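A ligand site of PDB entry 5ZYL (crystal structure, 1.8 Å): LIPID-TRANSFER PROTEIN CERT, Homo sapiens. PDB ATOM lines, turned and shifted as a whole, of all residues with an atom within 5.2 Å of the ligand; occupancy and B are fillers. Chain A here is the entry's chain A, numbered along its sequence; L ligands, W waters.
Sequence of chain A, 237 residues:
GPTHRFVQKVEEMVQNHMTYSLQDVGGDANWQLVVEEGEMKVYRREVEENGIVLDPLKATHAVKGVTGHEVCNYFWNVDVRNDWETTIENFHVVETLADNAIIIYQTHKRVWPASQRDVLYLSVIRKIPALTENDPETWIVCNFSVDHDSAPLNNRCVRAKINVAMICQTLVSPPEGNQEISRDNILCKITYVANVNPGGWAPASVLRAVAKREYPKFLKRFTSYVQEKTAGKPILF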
ATOM      1  N   PHE A  75      -0.518  25.443  -5.180  1.00  0.00           N
ATOM      2  CA  PHE A  75      -0.901  24.207  -5.842  1.00  0.00           C
ATOM      3  C   PHE A  75       0.338  23.399  -6.256  1.00  0.00           C
ATOM      4  O   PHE A  75       0.314  22.171  -6.309  1.00  0.00           O
ATOM      5  CB  PHE A  75      -1.782  24.546  -7.055  1.00  0.00           C
ATOM      6  CG  PHE A  75      -2.384  23.321  -7.734  1.00  0.00           C
ATOM      7  CD1 PHE A  75      -3.326  22.519  -7.077  1.00  0.00           C
ATOM      8  CD2 PHE A  75      -2.061  23.013  -9.029  1.00  0.00           C
ATOM      9  CE1 PHE A  75      -3.867  21.393  -7.697  1.00  0.00           C
ATOM     10  CE2 PHE A  75      -2.640  21.914  -9.670  1.00  0.00           C
ATOM     11  CZ  PHE A  75      -3.532  21.109  -9.004  1.00  0.00           C
ATOM     12  N   ARG A  81       1.709  20.278   0.235  1.00  0.00           N
ATOM     13  CA  ARG A  81       0.749  19.367  -0.346  1.00  0.00           C
ATOM     14  C   ARG A  81      -0.139  18.781   0.760  1.00  0.00           C
ATOM     15  O   ARG A  81      -1.346  18.717   0.598  1.00  0.00           O
ATOM     16  CB  ARG A  81       1.471  18.283  -1.162  1.00  0.00           C
ATOM     17  CG  ARG A  81       0.592  17.542  -2.161  1.00  0.00           C
ATOM     18  CD  ARG A  81       0.202  18.417  -3.352  1.00  0.00           C
ATOM     19  NE  ARG A  81       0.758  17.869  -4.584  1.00  0.00           N
ATOM     20  CZ  ARG A  81       1.491  18.537  -5.430  1.00  0.00           C
ATOM     21  NH1 ARG A  81       1.948  17.893  -6.503  1.00  0.00           N
ATOM     22  NH2 ARG A  81       1.744  19.831  -5.238  1.00  0.00           N
ATOM     23  N   TRP A  84      -3.426  20.441   2.241  1.00  0.00           N
ATOM     24  CA  TRP A  84      -4.715  20.540   1.575  1.00  0.00           C
ATOM     25  C   TRP A  84      -5.164  19.241   0.893  1.00  0.00           C
ATOM     26  O   TRP A  84      -6.360  19.064   0.722  1.00  0.00           O
ATOM     27  CB  TRP A  84      -4.796  21.725   0.590  1.00  0.00           C
ATOM     28  CG  TRP A  84      -3.772  21.672  -0.516  1.00  0.00           C
ATOM     29  CD1 TRP A  84      -2.553  22.292  -0.530  1.00  0.00           C
ATOM     30  CD2 TRP A  84      -3.881  20.984  -1.774  1.00  0.00           C
ATOM     31  NE1 TRP A  84      -1.890  22.030  -1.708  1.00  0.00           N
ATOM     32  CE2 TRP A  84      -2.689  21.228  -2.484  1.00  0.00           C
ATOM     33  CE3 TRP A  84      -4.880  20.168  -2.352  1.00  0.00           C
ATOM     34  CZ2 TRP A  84      -2.460  20.686  -3.749  1.00  0.00           C
ATOM     35  CZ3 TRP A  84      -4.631  19.610  -3.590  1.00  0.00           C
ATOM     36  CH2 TRP A  84      -3.454  19.887  -4.288  1.00  0.00           C
ATOM     37  N   GLU A  85      -4.219  18.352   0.486  1.00  0.00           N
ATOM     38  CA  GLU A  85      -4.588  17.092  -0.152  1.00  0.00           C
ATOM     39  C   GLU A  85      -5.258  16.175   0.858  1.00  0.00           C
ATOM     40  O   GLU A  85      -4.767  16.065   1.991  1.00  0.00           O
ATOM     41  CB  GLU A  85      -3.322  16.311  -0.526  1.00  0.00           C
ATOM     42  CG  GLU A  85      -2.619  16.792  -1.760  1.00  0.00           C
ATOM     43  CD  GLU A  85      -3.145  16.263  -3.080  1.00  0.00           C
ATOM     44  OE1 GLU A  85      -2.361  16.129  -4.009  1.00  0.00           O
ATOM     45  OE2 GLU A  85      -4.353  16.021  -3.169  1.00  0.00           O
ATOM     46  N   THR A  87      -6.580  12.923  -0.503  1.00  0.00           N
ATOM     47  CA  THR A  87      -6.758  11.611  -1.111  1.00  0.00           C
ATOM     48  C   THR A  87      -5.428  10.891  -1.410  1.00  0.00           C
ATOM     49  O   THR A  87      -5.468   9.796  -1.955  1.00  0.00           O
ATOM     50  CB  THR A  87      -7.613  11.669  -2.396  1.00  0.00           C
ATOM     51  OG1 THR A  87      -6.829  12.300  -3.416  1.00  0.00           O
ATOM     52  CG2 THR A  87      -8.912  12.445  -2.239  1.00  0.00           C
ATOM     53  N   ILE A  88      -4.286  11.496  -1.070  1.00  0.00           N
ATOM     54  CA  ILE A  88      -2.950  10.949  -1.318  1.00  0.00           C
ATOM     55  C   ILE A  88      -2.559  10.046  -0.177  1.00  0.00           C
ATOM     56  O   ILE A  88      -2.777  10.373   0.991  1.00  0.00           O
ATOM     57  CB  ILE A  88      -1.926  12.083  -1.497  1.00  0.00           C
ATOM     58  CG1 ILE A  88      -2.360  12.982  -2.646  1.00  0.00           C
ATOM     59  CG2 ILE A  88      -0.510  11.566  -1.735  1.00  0.00           C
ATOM     60  CD1 ILE A  88      -2.242  12.328  -3.929  1.00  0.00           C
ATOM     61  N   GLN A 106       2.877   9.382  -7.058  1.00  0.00           N
ATOM     62  CA  GLN A 106       2.006   9.385  -5.872  1.00  0.00           C
ATOM     63  C   GLN A 106       1.021   8.220  -5.961  1.00  0.00           C
ATOM     64  O   GLN A 106       0.754   7.709  -7.050  1.00  0.00           O
ATOM     65  CB  GLN A 106       1.247  10.694  -5.683  1.00  0.00           C
ATOM     66  CG  GLN A 106       0.309  11.046  -6.840  1.00  0.00           C
ATOM     67  CD  GLN A 106      -0.196  12.465  -6.726  1.00  0.00           C
ATOM     68  OE1 GLN A 106       0.564  13.389  -6.387  1.00  0.00           O
ATOM     69  NE2 GLN A 106      -1.450  12.692  -7.125  1.00  0.00           N
ATOM     70  N   HIS A 108      -2.999   7.142  -4.607  1.00  0.00           N
ATOM     71  CA  HIS A 108      -4.234   7.675  -4.050  1.00  0.00           C
ATOM     72  C   HIS A 108      -4.869   6.623  -3.166  1.00  0.00           C
ATOM     73  O   HIS A 108      -4.716   5.412  -3.370  1.00  0.00           O
ATOM     74  CB  HIS A 108      -5.194   8.056  -5.178  1.00  0.00           C
ATOM     75  CG  HIS A 108      -4.758   9.313  -5.839  1.00  0.00           C
ATOM     76  ND1 HIS A 108      -5.199  10.579  -5.438  1.00  0.00           N
ATOM     77  CD2 HIS A 108      -3.823   9.506  -6.797  1.00  0.00           C
ATOM     78  CE1 HIS A 108      -4.601  11.490  -6.191  1.00  0.00           C
ATOM     79  NE2 HIS A 108      -3.734  10.856  -7.001  1.00  0.00           N
ATOM     80  N   VAL A 111     -10.230   3.492  -3.870  1.00  0.00           N
ATOM     81  CA  VAL A 111     -11.659   3.697  -4.040  1.00  0.00           C
ATOM     82  C   VAL A 111     -12.299   2.335  -4.297  1.00  0.00           C
ATOM     83  O   VAL A 111     -12.127   1.769  -5.369  1.00  0.00           O
ATOM     84  CB  VAL A 111     -11.961   4.669  -5.181  1.00  0.00           C
ATOM     85  CG1 VAL A 111     -13.447   4.762  -5.468  1.00  0.00           C
ATOM     86  CG2 VAL A 111     -11.363   6.066  -4.903  1.00  0.00           C
ATOM     87  N   ARG A 117      -4.980   3.198  -7.182  1.00  0.00           N
ATOM     88  CA  ARG A 117      -4.302   3.779  -8.339  1.00  0.00           C
ATOM     89  C   ARG A 117      -3.010   4.478  -7.878  1.00  0.00           C
ATOM     90  O   ARG A 117      -2.984   5.122  -6.823  1.00  0.00           O
ATOM     91  CB  ARG A 117      -5.200   4.822  -9.039  1.00  0.00           C
ATOM     92  CG  ARG A 117      -5.877   4.318 -10.321  1.00  0.00           C
ATOM     93  CD  ARG A 117      -6.629   3.010 -10.102  1.00  0.00           C
ATOM     94  NE  ARG A 117      -7.245   2.538 -11.350  1.00  0.00           N
ATOM     95  CZ  ARG A 117      -7.978   1.431 -11.470  1.00  0.00           C
ATOM     96  NH1 ARG A 117      -8.263   0.717 -10.390  1.00  0.00           N
ATOM     97  NH2 ARG A 117      -8.402   1.052 -12.657  1.00  0.00           N
ATOM     98  N   VAL A 119       0.179   7.233  -9.832  1.00  0.00           N
ATOM     99  CA  VAL A 119       0.303   8.227 -10.902  1.00  0.00           C
ATOM    100  C   VAL A 119       1.751   8.666 -10.953  1.00  0.00           C
ATOM    101  O   VAL A 119       2.416   8.719  -9.930  1.00  0.00           O
ATOM    102  CB  VAL A 119      -0.542   9.472 -10.653  1.00  0.00           C
ATOM    103  CG1 VAL A 119      -0.802  10.197 -11.974  1.00  0.00           C
ATOM    104  CG2 VAL A 119      -1.859   9.099  -9.960  1.00  0.00           C
ATOM    105  N   TYR A 121       3.819  11.768 -12.864  1.00  0.00           N
ATOM    106  CA  TYR A 121       3.515  12.916 -13.700  1.00  0.00           C
ATOM    107  C   TYR A 121       4.577  14.008 -13.582  1.00  0.00           C
ATOM    108  O   TYR A 121       5.230  14.168 -12.563  1.00  0.00           O
ATOM    109  CB  TYR A 121       2.141  13.533 -13.377  1.00  0.00           C
ATOM    110  CG  TYR A 121       1.910  13.982 -11.943  1.00  0.00           C
ATOM    111  CD1 TYR A 121       1.634  13.083 -10.910  1.00  0.00           C
ATOM    112  CD2 TYR A 121       1.967  15.323 -11.617  1.00  0.00           C
ATOM    113  CE1 TYR A 121       1.372  13.506  -9.607  1.00  0.00           C
ATOM    114  CE2 TYR A 121       1.754  15.774 -10.308  1.00  0.00           C
ATOM    115  CZ  TYR A 121       1.467  14.865  -9.316  1.00  0.00           C
ATOM    116  OH  TYR A 121       1.241  15.320  -8.046  1.00  0.00           O
ATOM    117  N   ASN A 143      -0.149  19.425 -14.700  1.00  0.00           N
ATOM    118  CA  ASN A 143       0.356  18.148 -14.204  1.00  0.00           C
ATOM    119  C   ASN A 143      -0.050  17.089 -15.228  1.00  0.00           C
ATOM    120  O   ASN A 143      -1.242  16.856 -15.453  1.00  0.00           O
ATOM    121  CB  ASN A 143      -0.314  17.763 -12.867  1.00  0.00           C
ATOM    122  CG  ASN A 143       0.077  18.685 -11.723  1.00  0.00           C
ATOM    123  OD1 ASN A 143       1.174  19.241 -11.704  1.00  0.00           O
ATOM    124  ND2 ASN A 143      -0.800  18.840 -10.730  1.00  0.00           N
ATOM    125  N   ALA A 160      -2.795   5.068 -13.192  1.00  0.00           N
ATOM    126  CA  ALA A 160      -3.653   6.040 -13.867  1.00  0.00           C
ATOM    127  C   ALA A 160      -2.777   6.986 -14.667  1.00  0.00           C
ATOM    128  O   ALA A 160      -1.587   7.153 -14.345  1.00  0.00           O
ATOM    129  CB  ALA A 160      -4.447   6.789 -12.820  1.00  0.00           C
ATOM    130  N   ILE A 162      -2.869  11.142 -16.142  1.00  0.00           N
ATOM    131  CA  ILE A 162      -3.624  12.378 -15.900  1.00  0.00           C
ATOM    132  C   ILE A 162      -3.149  13.482 -16.833  1.00  0.00           C
ATOM    133  O   ILE A 162      -2.059  13.448 -17.370  1.00  0.00           O
ATOM    134  CB  ILE A 162      -3.535  12.847 -14.419  1.00  0.00           C
ATOM    135  CG1 ILE A 162      -2.106  13.266 -14.037  1.00  0.00           C
ATOM    136  CG2 ILE A 162      -4.055  11.753 -13.493  1.00  0.00           C
ATOM    137  CD1 ILE A 162      -1.980  13.963 -12.646  1.00  0.00           C
ATOM    138  N   VAL A 164      -3.942  17.512 -16.082  1.00  0.00           N
ATOM    139  CA  VAL A 164      -4.630  18.464 -15.224  1.00  0.00           C
ATOM    140  C   VAL A 164      -3.987  19.835 -15.433  1.00  0.00           C
ATOM    141  O   VAL A 164      -2.755  19.940 -15.551  1.00  0.00           O
ATOM    142  CB  VAL A 164      -4.478  18.026 -13.754  1.00  0.00           C
ATOM    143  CG1 VAL A 164      -4.890  19.143 -12.804  1.00  0.00           C
ATOM    144  CG2 VAL A 164      -5.251  16.737 -13.441  1.00  0.00           C
ATOM    145  N   TYR A 192     -10.087  25.098 -13.826  1.00  0.00           N
ATOM    146  CA  TYR A 192      -9.411  23.879 -13.420  1.00  0.00           C
ATOM    147  C   TYR A 192      -9.964  22.778 -14.340  1.00  0.00           C
ATOM    148  O   TYR A 192     -11.173  22.550 -14.427  1.00  0.00           O
ATOM    149  CB  TYR A 192      -9.745  23.533 -11.969  1.00  0.00           C
ATOM    150  CG  TYR A 192      -9.237  22.176 -11.555  1.00  0.00           C
ATOM    151  CD1 TYR A 192      -7.920  22.001 -11.161  1.00  0.00           C
ATOM    152  CD2 TYR A 192     -10.078  21.086 -11.508  1.00  0.00           C
ATOM    153  CE1 TYR A 192      -7.445  20.751 -10.773  1.00  0.00           C
ATOM    154  CE2 TYR A 192      -9.603  19.814 -11.202  1.00  0.00           C
ATOM    155  CZ  TYR A 192      -8.288  19.642 -10.786  1.00  0.00           C
ATOM    156  OH  TYR A 192      -7.843  18.390 -10.401  1.00  0.00           O
ATOM    157  N   VAL A 196      -8.592  12.390 -16.397  1.00  0.00           N
ATOM    158  CA  VAL A 196      -8.016  11.253 -15.682  1.00  0.00           C
ATOM    159  C   VAL A 196      -8.425   9.978 -16.386  1.00  0.00           C
ATOM    160  O   VAL A 196      -9.611   9.733 -16.623  1.00  0.00           O
ATOM    161  CB  VAL A 196      -8.498  11.219 -14.219  1.00  0.00           C
ATOM    162  CG1 VAL A 196      -7.896  10.038 -13.436  1.00  0.00           C
ATOM    163  CG2 VAL A 196      -8.150  12.512 -13.539  1.00  0.00           C
ATOM    164  N   PRO A 198      -8.291   6.131 -15.551  1.00  0.00           N
ATOM    165  CA  PRO A 198      -8.035   5.241 -14.423  1.00  0.00           C
ATOM    166  C   PRO A 198      -7.108   4.074 -14.775  1.00  0.00           C
ATOM    167  O   PRO A 198      -6.677   3.358 -13.877  1.00  0.00           O
ATOM    168  CB  PRO A 198      -9.428   4.675 -14.118  1.00  0.00           C
ATOM    169  CG  PRO A 198     -10.397   5.765 -14.583  1.00  0.00           C
ATOM    170  CD  PRO A 198      -9.733   6.249 -15.868  1.00  0.00           C
ATOM    171  N   LEU A 207     -16.983   5.610  -9.799  1.00  0.00           N
ATOM    172  CA  LEU A 207     -16.062   6.691 -10.137  1.00  0.00           C
ATOM    173  C   LEU A 207     -16.793   8.014 -10.334  1.00  0.00           C
ATOM    174  O   LEU A 207     -16.283   9.087  -9.997  1.00  0.00           O
ATOM    175  CB  LEU A 207     -15.311   6.314 -11.424  1.00  0.00           C
ATOM    176  CG  LEU A 207     -14.132   5.381 -11.233  1.00  0.00           C
ATOM    177  CD1 LEU A 207     -13.389   5.167 -12.555  1.00  0.00           C
ATOM    178  CD2 LEU A 207     -13.213   5.903 -10.140  1.00  0.00           C
ATOM    179  N   VAL A 210     -17.739   9.469  -7.037  1.00  0.00           N
ATOM    180  CA  VAL A 210     -16.564   9.955  -6.329  1.00  0.00           C
ATOM    181  C   VAL A 210     -16.087  11.294  -6.920  1.00  0.00           C
ATOM    182  O   VAL A 210     -15.769  12.225  -6.164  1.00  0.00           O
ATOM    183  CB  VAL A 210     -15.422   8.921  -6.299  1.00  0.00           C
ATOM    184  CG1 VAL A 210     -14.109   9.572  -5.929  1.00  0.00           C
ATOM    185  CG2 VAL A 210     -15.755   7.758  -5.382  1.00  0.00           C
ATOM    186  N   ALA A 211     -16.094  11.412  -8.260  1.00  0.00           N
ATOM    187  CA  ALA A 211     -15.689  12.656  -8.904  1.00  0.00           C
ATOM    188  C   ALA A 211     -16.640  13.777  -8.461  1.00  0.00           C
ATOM    189  O   ALA A 211     -16.223  14.892  -8.146  1.00  0.00           O
ATOM    190  CB  ALA A 211     -15.733  12.502 -10.419  1.00  0.00           C
ATOM    191  N   GLU A 214     -15.707  14.613  -4.838  1.00  0.00           N
ATOM    192  CA  GLU A 214     -14.345  14.991  -4.439  1.00  0.00           C
ATOM    193  C   GLU A 214     -13.853  16.242  -5.188  1.00  0.00           C
ATOM    194  O   GLU A 214     -13.030  16.985  -4.660  1.00  0.00           O
ATOM    195  CB  GLU A 214     -13.344  13.870  -4.703  1.00  0.00           C
ATOM    196  CG  GLU A 214     -13.535  12.657  -3.767  1.00  0.00           C
ATOM    197  CD  GLU A 214     -13.348  12.935  -2.272  1.00  0.00           C
ATOM    198  OE1 GLU A 214     -12.508  13.787  -1.914  1.00  0.00           O
ATOM    199  OE2 GLU A 214     -14.064  12.293  -1.447  1.00  0.00           O
ATOM    200  N   TYR A 215     -14.234  16.437  -6.454  1.00  0.00           N
ATOM    201  CA  TYR A 215     -13.694  17.624  -7.129  1.00  0.00           C
ATOM    202  C   TYR A 215     -14.177  18.914  -6.418  1.00  0.00           C
ATOM    203  O   TYR A 215     -13.385  19.845  -6.187  1.00  0.00           O
ATOM    204  CB  TYR A 215     -13.990  17.622  -8.623  1.00  0.00           C
ATOM    205  CG  TYR A 215     -13.066  16.714  -9.389  1.00  0.00           C
ATOM    206  CD1 TYR A 215     -11.729  17.038  -9.526  1.00  0.00           C
ATOM    207  CD2 TYR A 215     -13.524  15.572 -10.019  1.00  0.00           C
ATOM    208  CE1 TYR A 215     -10.839  16.231 -10.230  1.00  0.00           C
ATOM    209  CE2 TYR A 215     -12.650  14.749 -10.722  1.00  0.00           C
ATOM    210  CZ  TYR A 215     -11.307  15.069 -10.835  1.00  0.00           C
ATOM    211  OH  TYR A 215     -10.471  14.285 -11.580  1.00  0.00           O
ATOM    212  N   PHE A 218     -12.339  19.291  -3.082  1.00  0.00           N
ATOM    213  CA  PHE A 218     -10.968  19.745  -3.376  1.00  0.00           C
ATOM    214  C   PHE A 218     -10.942  21.245  -3.666  1.00  0.00           C
ATOM    215  O   PHE A 218     -10.138  21.954  -3.075  1.00  0.00           O
ATOM    216  CB  PHE A 218     -10.337  18.939  -4.519  1.00  0.00           C
ATOM    217  CG  PHE A 218      -9.305  19.706  -5.333  1.00  0.00           C
ATOM    218  CD1 PHE A 218      -8.153  20.194  -4.746  1.00  0.00           C
ATOM    219  CD2 PHE A 218      -9.549  20.003  -6.672  1.00  0.00           C
ATOM    220  CE1 PHE A 218      -7.222  20.910  -5.504  1.00  0.00           C
ATOM    221  CE2 PHE A 218      -8.644  20.756  -7.411  1.00  0.00           C
ATOM    222  CZ  PHE A 218      -7.484  21.208  -6.818  1.00  0.00           C
HETATM  223  C1  LIG L   1      -8.890   7.225 -10.793  1.00  0.00           C
HETATM  224  C2  LIG L   1      -6.464  15.550  -8.903  1.00  0.00           C
HETATM  225  C3  LIG L   1      -2.204  16.634  -7.335  1.00  0.00           C
HETATM  226  C4  LIG L   1      -3.431  17.541  -7.587  1.00  0.00           C
HETATM  227  C5  LIG L   1      -5.083  15.593  -9.237  1.00  0.00           C
HETATM  228  C6  LIG L   1      -7.097  11.841  -9.418  1.00  0.00           C
HETATM  229  C7  LIG L   1      -8.497  11.773  -9.533  1.00  0.00           C
HETATM  230  C8  LIG L   1     -10.753  10.675  -9.662  1.00  0.00           C
HETATM  231  C9  LIG L   1      -9.242  10.596  -9.584  1.00  0.00           C
HETATM  232  N1  LIG L   1      -9.924  11.850  -6.805  1.00  0.00           N
HETATM  233  C10 LIG L   1      -9.351   5.766 -10.477  1.00  0.00           C
HETATM  234  C11 LIG L   1      -8.543   9.369  -9.515  1.00  0.00           C
HETATM  235  C12 LIG L   1      -7.120   9.408  -9.430  1.00  0.00           C
HETATM  236  C13 LIG L   1      -6.396  13.136  -9.372  1.00  0.00           C
HETATM  237  O1  LIG L   1      -5.370  18.145  -9.360  1.00  0.00           O
HETATM  238  S1  LIG L   1      -4.243  17.184  -9.221  1.00  0.00           S
HETATM  239  O2  LIG L   1      -3.200  17.088 -10.227  1.00  0.00           O
HETATM  240  O3  LIG L   1      -2.697  15.364  -6.870  1.00  0.00           O
HETATM  241  C14 LIG L   1      -4.326  14.447  -9.593  1.00  0.00           C
HETATM  242  C15 LIG L   1      -5.008  13.200  -9.654  1.00  0.00           C
HETATM  243  C16 LIG L   1      -7.100  14.314  -8.996  1.00  0.00           C
HETATM  244  C17 LIG L   1      -6.381  10.626  -9.372  1.00  0.00           C
HETATM  245  C18 LIG L   1      -9.317   8.047  -9.588  1.00  0.00           C
HETATM  246  C19 LIG L   1      -9.121   7.065  -8.385  1.00  0.00           C
HETATM  247  C20 LIG L   1      -9.494   5.686  -8.950  1.00  0.00           C
HETATM  248  C21 LIG L   1     -11.495  11.585  -8.680  1.00  0.00           C
HETATM  249  C22 LIG L   1     -11.545  10.063  -8.540  1.00  0.00           C
HETATM  250  C23 LIG L   1     -10.780  12.464  -7.680  1.00  0.00           C
HETATM  251  C24 LIG L   1     -10.980  13.851  -7.581  1.00  0.00           C
HETATM  252  C25 LIG L   1     -10.279  14.626  -6.620  1.00  0.00           C
HETATM  253  C26 LIG L   1      -9.349  13.967  -5.767  1.00  0.00           C
HETATM  254  C27 LIG L   1      -9.230  12.554  -5.907  1.00  0.00           C
HETATM  255  O   HOH W   1      -7.505  16.928  -5.832  1.00  0.00           O
HETATM  256  O   HOH W   2      -5.284  15.134  -5.787  1.00  0.00           O
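Phe 75 touches the ligand. Thr 87 touches the ligand. NE2 of His 108 touches C17 of the ligand, 3.6 Å away. CG of Arg 117 touches C10 of the ligand, at 3.8 Å. Tyr 121 touches the ligand. Ile 162 touches the ligand (CD1 to C14, 3.9 Å). Val 164 touches the ligand. Val 196 touches the ligand (CG1 to C1, 3.99 Å). Pro 198 touches the ligand (CB to C10, 3.8 Å). Leu 207 touches the ligand. Val 210 touches the ligand (CG1 to C22, 3.7 Å). CB of Glu 214 touches C25 of the ligand (3.7 Å). Tyr 215 touches the ligand (CZ to C24, 3.5 Å). Of the 25 residues printed, 17 come within 4 Å of the ligand. The nearest printed residue that does not touch the ligand is Trp 84 (4.05 Å).
OE1 of Gln 106 lies within hydrogen-bond range of OH of Tyr 121, at 2.6 Å. The side-chain carboxylate (OE1) of Glu 85 lies within salt-bridge range of the guanidinium group (NE) of Arg 81 (3.6 Å). A ring nitrogen (NE2) of His 108 sits at hydrogen-bond distance from the side-chain amide nitrogen of Gln 106 (2.9 Å). The backbone NH (N) of Asn 143 sits at hydrogen-bond distance from the backbone carbonyl oxygen (O) of Val 164, at 2.8 Å. OH of Tyr 121 sits at hydrogen-bond distance from NH1 of Arg 81. The backbone carbonyl oxygen (O) of Arg 117 lies within hydrogen-bond range of the backbone NH (N) of His 108 (3.0 Å). The backbone carbonyl oxygen (O) of Gln 106 sits at hydrogen-bond distance from the backbone NH (N) of Val 119 (2.9 Å). The backbone carbonyl oxygen of Phe 75 lies within hydrogen-bond range of the guanidinium group of Arg 81, 2.9 Å away.
The side-chain amide nitrogen of Asn 143 lies within hydrogen-bond range of an oxygen (O2) of the ligand, at 3.0 Å. An oxygen (O3) of the ligand lies within hydrogen-bond range of the side-chain amide nitrogen (NE2) of Gln 106. O1 of the ligand sits at hydrogen-bond distance from OH of Tyr 192 (2.7 Å). OE1 of Glu 85 is in hydrogen-bond range of O3 of the ligand (3.0 Å).
Water W2 bridges O3 of the ligand and OE2 of Glu 85.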
